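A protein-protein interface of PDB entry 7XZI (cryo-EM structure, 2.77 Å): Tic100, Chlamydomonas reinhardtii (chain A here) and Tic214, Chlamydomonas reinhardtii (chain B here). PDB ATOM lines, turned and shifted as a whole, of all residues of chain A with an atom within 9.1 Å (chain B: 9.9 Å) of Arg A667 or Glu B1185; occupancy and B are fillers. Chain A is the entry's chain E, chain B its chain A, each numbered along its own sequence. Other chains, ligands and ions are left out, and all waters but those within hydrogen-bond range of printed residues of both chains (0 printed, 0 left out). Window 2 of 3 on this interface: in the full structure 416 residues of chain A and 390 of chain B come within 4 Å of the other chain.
The side-chain carboxylate of Asp A664 is in salt-bridge range of the guanidinium group of Arg A667 (3.8 Å).
OD1 of Asn B584 sits close to O of Leu B1181.
OD1 of Asn B584 sits at hydrogen-bond distance from N of Glu B1185.
The side-chain hydroxyl of Thr B1182 is in hydrogen-bond range of the backbone carbonyl oxygen of Ile B1178, at 2.6 Å.
Among the printed residues, pairs that only touch across the chains: Val A660 with Asn B1179 (3.2 Å), Asp A664 with Thr B1182 (3.3 Å), Phe A443 with Leu B1181 (3.4 Å), Arg A667 with Glu B1185 (3.5 Å), Phe A443 with Ile B1178 (3.6 Å), Arg A667 with Thr B1182 (3.6 Å), Val A668 with Ile B1178 (3.7 Å), Val A660 with Ile B1178 (3.7 Å), Leu A671 with Leu B583 (3.8 Å), Phe A443 with Val B1177 (3.8 Å), Val A668 with Leu B1181 (3.8 Å) and Phe A443 with Leu B583 (3.9 Å).
Printed residues of chain B within 4 Å of Phe A443: Leu B583 (3.9 Å), Val B1177 (3.8 Å), Ile B1178 (3.6 Å) and Leu B1181 (3.4 Å).
Asp A664 touches just one residue of chain B: Thr B1182.
No residue of chain B comes within 4 Å of Glu A665.
No residue of chain B comes within 4 Å of Arg A666.
Of chain B, only Thr B1182 and Glu B1185 come within 4 Å of Arg A667.
Of chain B, only Ile B1178 (3.7 Å) and Leu B1181 (3.8 Å) come within 4 Å of Val A668.
No residue of chain B comes within 4 Å of Glu A669.
No residue of chain B comes within 4 Å of Gly A670.
Ala A672 touches none of the printed residues of chain B.
Trp A675 touches none of the printed residues of chain B.
Of the printed residues of chain A, Leu B583 touches Phe A443 (3.9 Å) and Leu A671 (3.8 Å).
Printed residues of chain A within 4 Å of Val B1177: Phe A443.
Of the printed residues of chain A, Asn B1179 touches Val A660.
Printed residues of chain A within 4 Å of Thr B1182: Asp A664 and Arg A667.
Asn B1184 touches none of the printed residues of chain A.
Glu B1185 touches just one residue of chain A: Arg A667 (3.5 Å).
The nearest residue of chain B that does not touch Arg A667 is Leu B1181 (5.9 Å).
The nearest residue of chain A that does not touch Glu B1185 is Leu A671 (5.5 Å).
The nearest printed residue of chain B that does not touch Leu A671 is Ser B585 (5.2 Å).
Printed residues of chain A that touch a printed residue of chain B: Phe A443, Val A660, Asp A664, Arg A667, Val A668 and Leu A671.
Hydrophobic or aromatic side chains of chain A within 4 Å of the printed part of chain B: Phe A443, Val A660, Val A668 and Leu A671.
Printed residues of chain B that touch a printed residue of chain A: Leu B583, Val B1177, Ile B1178, Asn B1179, Leu B1181, Thr B1182 and Glu B1185.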
ATOM      1  N   PHE A 443      18.773   7.722   9.922  1.00  0.00           N
ATOM      2  CA  PHE A 443      17.521   7.314  10.553  1.00  0.00           C
ATOM      3  C   PHE A 443      16.430   8.355  10.351  1.00  0.00           C
ATOM      4  O   PHE A 443      15.279   8.012  10.050  1.00  0.00           O
ATOM      5  CB  PHE A 443      17.740   7.054  12.043  1.00  0.00           C
ATOM      6  CG  PHE A 443      16.497   6.631  12.771  1.00  0.00           C
ATOM      7  CD1 PHE A 443      15.965   5.370  12.579  1.00  0.00           C
ATOM      8  CD2 PHE A 443      15.859   7.496  13.645  1.00  0.00           C
ATOM      9  CE1 PHE A 443      14.822   4.975  13.243  1.00  0.00           C
ATOM     10  CE2 PHE A 443      14.713   7.105  14.312  1.00  0.00           C
ATOM     11  CZ  PHE A 443      14.195   5.842  14.110  1.00  0.00           C
ATOM     12  N   VAL A 660       8.365  -4.715  19.247  1.00  0.00           N
ATOM     13  CA  VAL A 660       9.558  -3.890  19.390  1.00  0.00           C
ATOM     14  C   VAL A 660       9.748  -3.602  20.872  1.00  0.00           C
ATOM     15  O   VAL A 660       8.951  -2.878  21.481  1.00  0.00           O
ATOM     16  CB  VAL A 660       9.454  -2.588  18.584  1.00  0.00           C
ATOM     17  CG1 VAL A 660      10.708  -1.751  18.771  1.00  0.00           C
ATOM     18  CG2 VAL A 660       9.220  -2.890  17.114  1.00  0.00           C
ATOM     19  N   SER A 661      10.801  -4.166  21.456  1.00  0.00           N
ATOM     20  CA  SER A 661      11.117  -3.898  22.849  1.00  0.00           C
ATOM     21  C   SER A 661      11.805  -2.543  22.994  1.00  0.00           C
ATOM     22  O   SER A 661      12.337  -1.978  22.034  1.00  0.00           O
ATOM     23  CB  SER A 661      12.007  -5.003  23.419  1.00  0.00           C
ATOM     24  OG  SER A 661      12.352  -4.732  24.766  1.00  0.00           O
ATOM     25  N   LYS A 662      11.787  -2.018  24.222  1.00  0.00           N
ATOM     26  CA  LYS A 662      12.470  -0.762  24.504  1.00  0.00           C
ATOM     27  C   LYS A 662      13.980  -0.885  24.364  1.00  0.00           C
ATOM     28  O   LYS A 662      14.651   0.117  24.088  1.00  0.00           O
ATOM     29  CB  LYS A 662      12.116  -0.271  25.909  1.00  0.00           C
ATOM     30  N   GLU A 663      14.528  -2.089  24.550  1.00  0.00           N
ATOM     31  CA  GLU A 663      15.957  -2.293  24.344  1.00  0.00           C
ATOM     32  C   GLU A 663      16.340  -2.046  22.891  1.00  0.00           C
ATOM     33  O   GLU A 663      17.394  -1.464  22.611  1.00  0.00           O
ATOM     34  CB  GLU A 663      16.352  -3.706  24.774  1.00  0.00           C
ATOM     35  N   ASP A 664      15.497  -2.481  21.952  1.00  0.00           N
ATOM     36  CA  ASP A 664      15.759  -2.219  20.539  1.00  0.00           C
ATOM     37  C   ASP A 664      15.748  -0.725  20.244  1.00  0.00           C
ATOM     38  O   ASP A 664      16.602  -0.223  19.503  1.00  0.00           O
ATOM     39  CB  ASP A 664      14.728  -2.942  19.671  1.00  0.00           C
ATOM     40  CG  ASP A 664      14.696  -4.435  19.924  1.00  0.00           C
ATOM     41  OD1 ASP A 664      14.335  -4.841  21.048  1.00  0.00           O
ATOM     42  OD2 ASP A 664      15.027  -5.205  18.997  1.00  0.00           O
ATOM     43  N   GLU A 665      14.781   0.002  20.811  1.00  0.00           N
ATOM     44  CA  GLU A 665      14.723   1.446  20.607  1.00  0.00           C
ATOM     45  C   GLU A 665      15.955   2.131  21.182  1.00  0.00           C
ATOM     46  O   GLU A 665      16.524   3.033  20.556  1.00  0.00           O
ATOM     47  CB  GLU A 665      13.450   2.015  21.234  1.00  0.00           C
ATOM     48  N   ARG A 666      16.383   1.714  22.377  1.00  0.00           N
ATOM     49  CA  ARG A 666      17.587   2.283  22.973  1.00  0.00           C
ATOM     50  C   ARG A 666      18.817   1.984  22.123  1.00  0.00           C
ATOM     51  O   ARG A 666      19.681   2.849  21.942  1.00  0.00           O
ATOM     52  CB  ARG A 666      17.771   1.749  24.394  1.00  0.00           C
ATOM     53  N   ARG A 667      18.911   0.761  21.595  1.00  0.00           N
ATOM     54  CA  ARG A 667      20.038   0.401  20.740  1.00  0.00           C
ATOM     55  C   ARG A 667      20.064   1.248  19.475  1.00  0.00           C
ATOM     56  O   ARG A 667      21.128   1.726  19.063  1.00  0.00           O
ATOM     57  CB  ARG A 667      19.967  -1.084  20.383  1.00  0.00           C
ATOM     58  CG  ARG A 667      21.092  -1.562  19.479  1.00  0.00           C
ATOM     59  CD  ARG A 667      20.604  -2.624  18.507  1.00  0.00           C
ATOM     60  NE  ARG A 667      19.965  -3.742  19.186  1.00  0.00           N
ATOM     61  CZ  ARG A 667      19.373  -4.757  18.565  1.00  0.00           C
ATOM     62  NH1 ARG A 667      19.323  -4.824  17.244  1.00  0.00           N
ATOM     63  NH2 ARG A 667      18.817  -5.724  19.287  1.00  0.00           N
ATOM     64  N   VAL A 668      18.904   1.445  18.847  1.00  0.00           N
ATOM     65  CA  VAL A 668      18.850   2.249  17.630  1.00  0.00           C
ATOM     66  C   VAL A 668      19.194   3.703  17.931  1.00  0.00           C
ATOM     67  O   VAL A 668      19.900   4.361  17.156  1.00  0.00           O
ATOM     68  CB  VAL A 668      17.470   2.117  16.960  1.00  0.00           C
ATOM     69  CG1 VAL A 668      17.363   3.063  15.775  1.00  0.00           C
ATOM     70  CG2 VAL A 668      17.237   0.684  16.513  1.00  0.00           C
ATOM     71  N   GLU A 669      18.702   4.228  19.056  1.00  0.00           N
ATOM     72  CA  GLU A 669      19.025   5.601  19.430  1.00  0.00           C
ATOM     73  C   GLU A 669      20.519   5.766  19.683  1.00  0.00           C
ATOM     74  O   GLU A 669      21.121   6.761  19.262  1.00  0.00           O
ATOM     75  CB  GLU A 669      18.222   6.012  20.663  1.00  0.00           C
ATOM     76  N   GLY A 670      21.133   4.800  20.370  1.00  0.00           N
ATOM     77  CA  GLY A 670      22.571   4.856  20.579  1.00  0.00           C
ATOM     78  C   GLY A 670      23.351   4.767  19.283  1.00  0.00           C
ATOM     79  O   GLY A 670      24.337   5.482  19.090  1.00  0.00           O
ATOM     80  N   LEU A 671      22.916   3.892  18.372  1.00  0.00           N
ATOM     81  CA  LEU A 671      23.573   3.779  17.074  1.00  0.00           C
ATOM     82  C   LEU A 671      23.485   5.090  16.303  1.00  0.00           C
ATOM     83  O   LEU A 671      24.463   5.524  15.685  1.00  0.00           O
ATOM     84  CB  LEU A 671      22.948   2.636  16.272  1.00  0.00           C
ATOM     85  CG  LEU A 671      23.809   1.828  15.293  1.00  0.00           C
ATOM     86  CD1 LEU A 671      23.044   0.604  14.805  1.00  0.00           C
ATOM     87  CD2 LEU A 671      24.273   2.666  14.110  1.00  0.00           C
ATOM     88  N   ALA A 672      22.318   5.736  16.330  1.00  0.00           N
ATOM     89  CA  ALA A 672      22.151   6.988  15.603  1.00  0.00           C
ATOM     90  C   ALA A 672      22.966   8.115  16.228  1.00  0.00           C
ATOM     91  O   ALA A 672      23.622   8.881  15.514  1.00  0.00           O
ATOM     92  CB  ALA A 672      20.671   7.367  15.543  1.00  0.00           C
ATOM     93  N   ALA A 673      22.946   8.227  17.558  1.00  0.00           N
ATOM     94  CA  ALA A 673      23.568   9.371  18.218  1.00  0.00           C
ATOM     95  C   ALA A 673      25.071   9.178  18.398  1.00  0.00           C
ATOM     96  O   ALA A 673      25.875   9.955  17.874  1.00  0.00           O
ATOM     97  CB  ALA A 673      22.893   9.623  19.569  1.00  0.00           C
ATOM     98  N   ARG A 674      25.467   8.141  19.142  1.00  0.00           N
ATOM     99  CA  ARG A 674      26.869   7.998  19.517  1.00  0.00           C
ATOM    100  C   ARG A 674      27.733   7.517  18.359  1.00  0.00           C
ATOM    101  O   ARG A 674      28.905   7.899  18.266  1.00  0.00           O
ATOM    102  N   TRP A 675      27.185   6.687  17.474  1.00  0.00           N
ATOM    103  CA  TRP A 675      27.959   6.095  16.390  1.00  0.00           C
ATOM    104  C   TRP A 675      27.877   6.886  15.092  1.00  0.00           C
ATOM    105  O   TRP A 675      28.837   6.887  14.316  1.00  0.00           O
ATOM    106  CB  TRP A 675      27.499   4.656  16.136  1.00  0.00           C
ATOM    107  N   LEU B 580      19.022   3.014   4.673  1.00  0.00           N
ATOM    108  CA  LEU B 580      18.786   1.811   5.466  1.00  0.00           C
ATOM    109  C   LEU B 580      19.951   0.838   5.343  1.00  0.00           C
ATOM    110  O   LEU B 580      20.375   0.230   6.333  1.00  0.00           O
ATOM    111  CB  LEU B 580      17.473   1.151   5.041  1.00  0.00           C
ATOM    112  CG  LEU B 580      16.928   0.041   5.946  1.00  0.00           C
ATOM    113  CD1 LEU B 580      15.409   0.073   5.965  1.00  0.00           C
ATOM    114  CD2 LEU B 580      17.420  -1.331   5.506  1.00  0.00           C
ATOM    115  N   LYS B 581      20.480   0.671   4.128  1.00  0.00           N
ATOM    116  CA  LYS B 581      21.629  -0.206   3.933  1.00  0.00           C
ATOM    117  C   LYS B 581      22.846   0.306   4.691  1.00  0.00           C
ATOM    118  O   LYS B 581      23.563  -0.475   5.324  1.00  0.00           O
ATOM    119  CB  LYS B 581      21.939  -0.334   2.441  1.00  0.00           C
ATOM    120  CG  LYS B 581      23.136  -1.214   2.119  1.00  0.00           C
ATOM    121  CD  LYS B 581      22.805  -2.688   2.275  1.00  0.00           C
ATOM    122  CE  LYS B 581      23.969  -3.562   1.830  1.00  0.00           C
ATOM    123  NZ  LYS B 581      23.629  -5.010   1.880  1.00  0.00           N
ATOM    124  N   LEU B 583      22.881   2.211   7.393  1.00  0.00           N
ATOM    125  CA  LEU B 583      22.676   2.142   8.834  1.00  0.00           C
ATOM    126  C   LEU B 583      22.684   0.714   9.368  1.00  0.00           C
ATOM    127  O   LEU B 583      22.816   0.522  10.581  1.00  0.00           O
ATOM    128  CB  LEU B 583      21.361   2.832   9.207  1.00  0.00           C
ATOM    129  CG  LEU B 583      21.197   3.259  10.667  1.00  0.00           C
ATOM    130  CD1 LEU B 583      22.417   4.037  11.124  1.00  0.00           C
ATOM    131  CD2 LEU B 583      19.938   4.088  10.847  1.00  0.00           C
ATOM    132  N   ASN B 584      22.549  -0.288   8.497  1.00  0.00           N
ATOM    133  CA  ASN B 584      22.537  -1.690   8.914  1.00  0.00           C
ATOM    134  C   ASN B 584      23.964  -2.223   9.083  1.00  0.00           C
ATOM    135  O   ASN B 584      24.377  -3.203   8.462  1.00  0.00           O
ATOM    136  CB  ASN B 584      21.750  -2.528   7.915  1.00  0.00           C
ATOM    137  CG  ASN B 584      20.472  -3.087   8.505  1.00  0.00           C
ATOM    138  OD1 ASN B 584      20.365  -3.278   9.716  1.00  0.00           O
ATOM    139  ND2 ASN B 584      19.491  -3.357   7.649  1.00  0.00           N
ATOM    140  N   SER B 585      24.718  -1.543   9.949  1.00  0.00           N
ATOM    141  CA  SER B 585      26.097  -1.916  10.279  1.00  0.00           C
ATOM    142  C   SER B 585      26.996  -1.936   9.045  1.00  0.00           C
ATOM    143  O   SER B 585      28.042  -2.590   9.033  1.00  0.00           O
ATOM    144  CB  SER B 585      26.151  -3.263  11.005  1.00  0.00           C
ATOM    145  OG  SER B 585      25.469  -3.206  12.245  1.00  0.00           O
ATOM    146  N   LYS B 586      26.598  -1.221   7.991  1.00  0.00           N
ATOM    147  CA  LYS B 586      27.458  -1.089   6.823  1.00  0.00           C
ATOM    148  C   LYS B 586      28.566  -0.071   7.037  1.00  0.00           C
ATOM    149  O   LYS B 586      29.554  -0.081   6.295  1.00  0.00           O
ATOM    150  CB  LYS B 586      26.638  -0.701   5.593  1.00  0.00           C
ATOM    151  N   VAL B1177       9.899   1.366  10.845  1.00  0.00           N
ATOM    152  CA  VAL B1177      11.287   1.687  10.517  1.00  0.00           C
ATOM    153  C   VAL B1177      12.240   1.003  11.494  1.00  0.00           C
ATOM    154  O   VAL B1177      13.303   0.501  11.103  1.00  0.00           O
ATOM    155  CB  VAL B1177      11.498   3.212  10.491  1.00  0.00           C
ATOM    156  CG1 VAL B1177      12.958   3.542  10.222  1.00  0.00           C
ATOM    157  CG2 VAL B1177      10.608   3.850   9.438  1.00  0.00           C
ATOM    158  N   ILE B1178      11.876   0.972  12.779  1.00  0.00           N
ATOM    159  CA  ILE B1178      12.717   0.322  13.781  1.00  0.00           C
ATOM    160  C   ILE B1178      12.842  -1.169  13.493  1.00  0.00           C
ATOM    161  O   ILE B1178      13.924  -1.749  13.622  1.00  0.00           O
ATOM    162  CB  ILE B1178      12.166   0.579  15.197  1.00  0.00           C
ATOM    163  CG1 ILE B1178      12.317   2.054  15.574  1.00  0.00           C
ATOM    164  CG2 ILE B1178      12.883  -0.289  16.214  1.00  0.00           C
ATOM    165  CD1 ILE B1178      13.749   2.517  15.650  1.00  0.00           C
ATOM    166  N   ASN B1179      11.736  -1.815  13.117  1.00  0.00           N
ATOM    167  CA  ASN B1179      11.786  -3.232  12.763  1.00  0.00           C
ATOM    168  C   ASN B1179      12.674  -3.465  11.548  1.00  0.00           C
ATOM    169  O   ASN B1179      13.456  -4.424  11.513  1.00  0.00           O
ATOM    170  CB  ASN B1179      10.378  -3.763  12.498  1.00  0.00           C
ATOM    171  CG  ASN B1179       9.662  -4.178  13.766  1.00  0.00           C
ATOM    172  OD1 ASN B1179      10.273  -4.718  14.687  1.00  0.00           O
ATOM    173  ND2 ASN B1179       8.359  -3.933  13.816  1.00  0.00           N
ATOM    174  N   GLN B1180      12.559  -2.600  10.536  1.00  0.00           N
ATOM    175  CA  GLN B1180      13.400  -2.738   9.351  1.00  0.00           C
ATOM    176  C   GLN B1180      14.875  -2.624   9.710  1.00  0.00           C
ATOM    177  O   GLN B1180      15.708  -3.375   9.191  1.00  0.00           O
ATOM    178  CB  GLN B1180      13.022  -1.690   8.305  1.00  0.00           C
ATOM    179  CG  GLN B1180      11.651  -1.896   7.690  1.00  0.00           C
ATOM    180  CD  GLN B1180      11.344  -0.888   6.602  1.00  0.00           C
ATOM    181  OE1 GLN B1180      12.157  -0.013   6.300  1.00  0.00           O
ATOM    182  NE2 GLN B1180      10.164  -1.005   6.006  1.00  0.00           N
ATOM    183  N   LEU B1181      15.219  -1.681  10.590  1.00  0.00           N
ATOM    184  CA  LEU B1181      16.604  -1.561  11.033  1.00  0.00           C
ATOM    185  C   LEU B1181      17.044  -2.784  11.832  1.00  0.00           C
ATOM    186  O   LEU B1181      18.153  -3.295  11.637  1.00  0.00           O
ATOM    187  CB  LEU B1181      16.787  -0.294  11.864  1.00  0.00           C
ATOM    188  CG  LEU B1181      16.852   1.022  11.094  1.00  0.00           C
ATOM    189  CD1 LEU B1181      17.092   2.164  12.055  1.00  0.00           C
ATOM    190  CD2 LEU B1181      17.946   0.963  10.042  1.00  0.00           C
ATOM    191  N   THR B1182      16.189  -3.266  12.736  1.00  0.00           N
ATOM    192  CA  THR B1182      16.566  -4.362  13.621  1.00  0.00           C
ATOM    193  C   THR B1182      16.733  -5.671  12.861  1.00  0.00           C
ATOM    194  O   THR B1182      17.478  -6.551  13.307  1.00  0.00           O
ATOM    195  CB  THR B1182      15.525  -4.520  14.731  1.00  0.00           C
ATOM    196  OG1 THR B1182      15.244  -3.239  15.308  1.00  0.00           O
ATOM    197  CG2 THR B1182      16.035  -5.449  15.825  1.00  0.00           C
ATOM    198  N   ASN B1183      16.048  -5.818  11.723  1.00  0.00           N
ATOM    199  CA  ASN B1183      16.182  -7.034  10.924  1.00  0.00           C
ATOM    200  C   ASN B1183      17.645  -7.345  10.626  1.00  0.00           C
ATOM    201  O   ASN B1183      18.107  -8.474  10.825  1.00  0.00           O
ATOM    202  CB  ASN B1183      15.387  -6.895   9.625  1.00  0.00           C
ATOM    203  N   ASN B1184      18.392  -6.347  10.154  1.00  0.00           N
ATOM    204  CA  ASN B1184      19.814  -6.544   9.885  1.00  0.00           C
ATOM    205  C   ASN B1184      20.632  -6.587  11.170  1.00  0.00           C
ATOM    206  O   ASN B1184      21.564  -7.389  11.289  1.00  0.00           O
ATOM    207  N   GLU B1185      20.304  -5.733  12.135  1.00  0.00           N
ATOM    208  CA  GLU B1185      21.051  -5.665  13.386  1.00  0.00           C
ATOM    209  C   GLU B1185      20.753  -6.864  14.280  1.00  0.00           C
ATOM    210  O   GLU B1185      21.588  -7.273  15.087  1.00  0.00           O
ATOM    211  CB  GLU B1185      20.735  -4.365  14.129  1.00  0.00           C
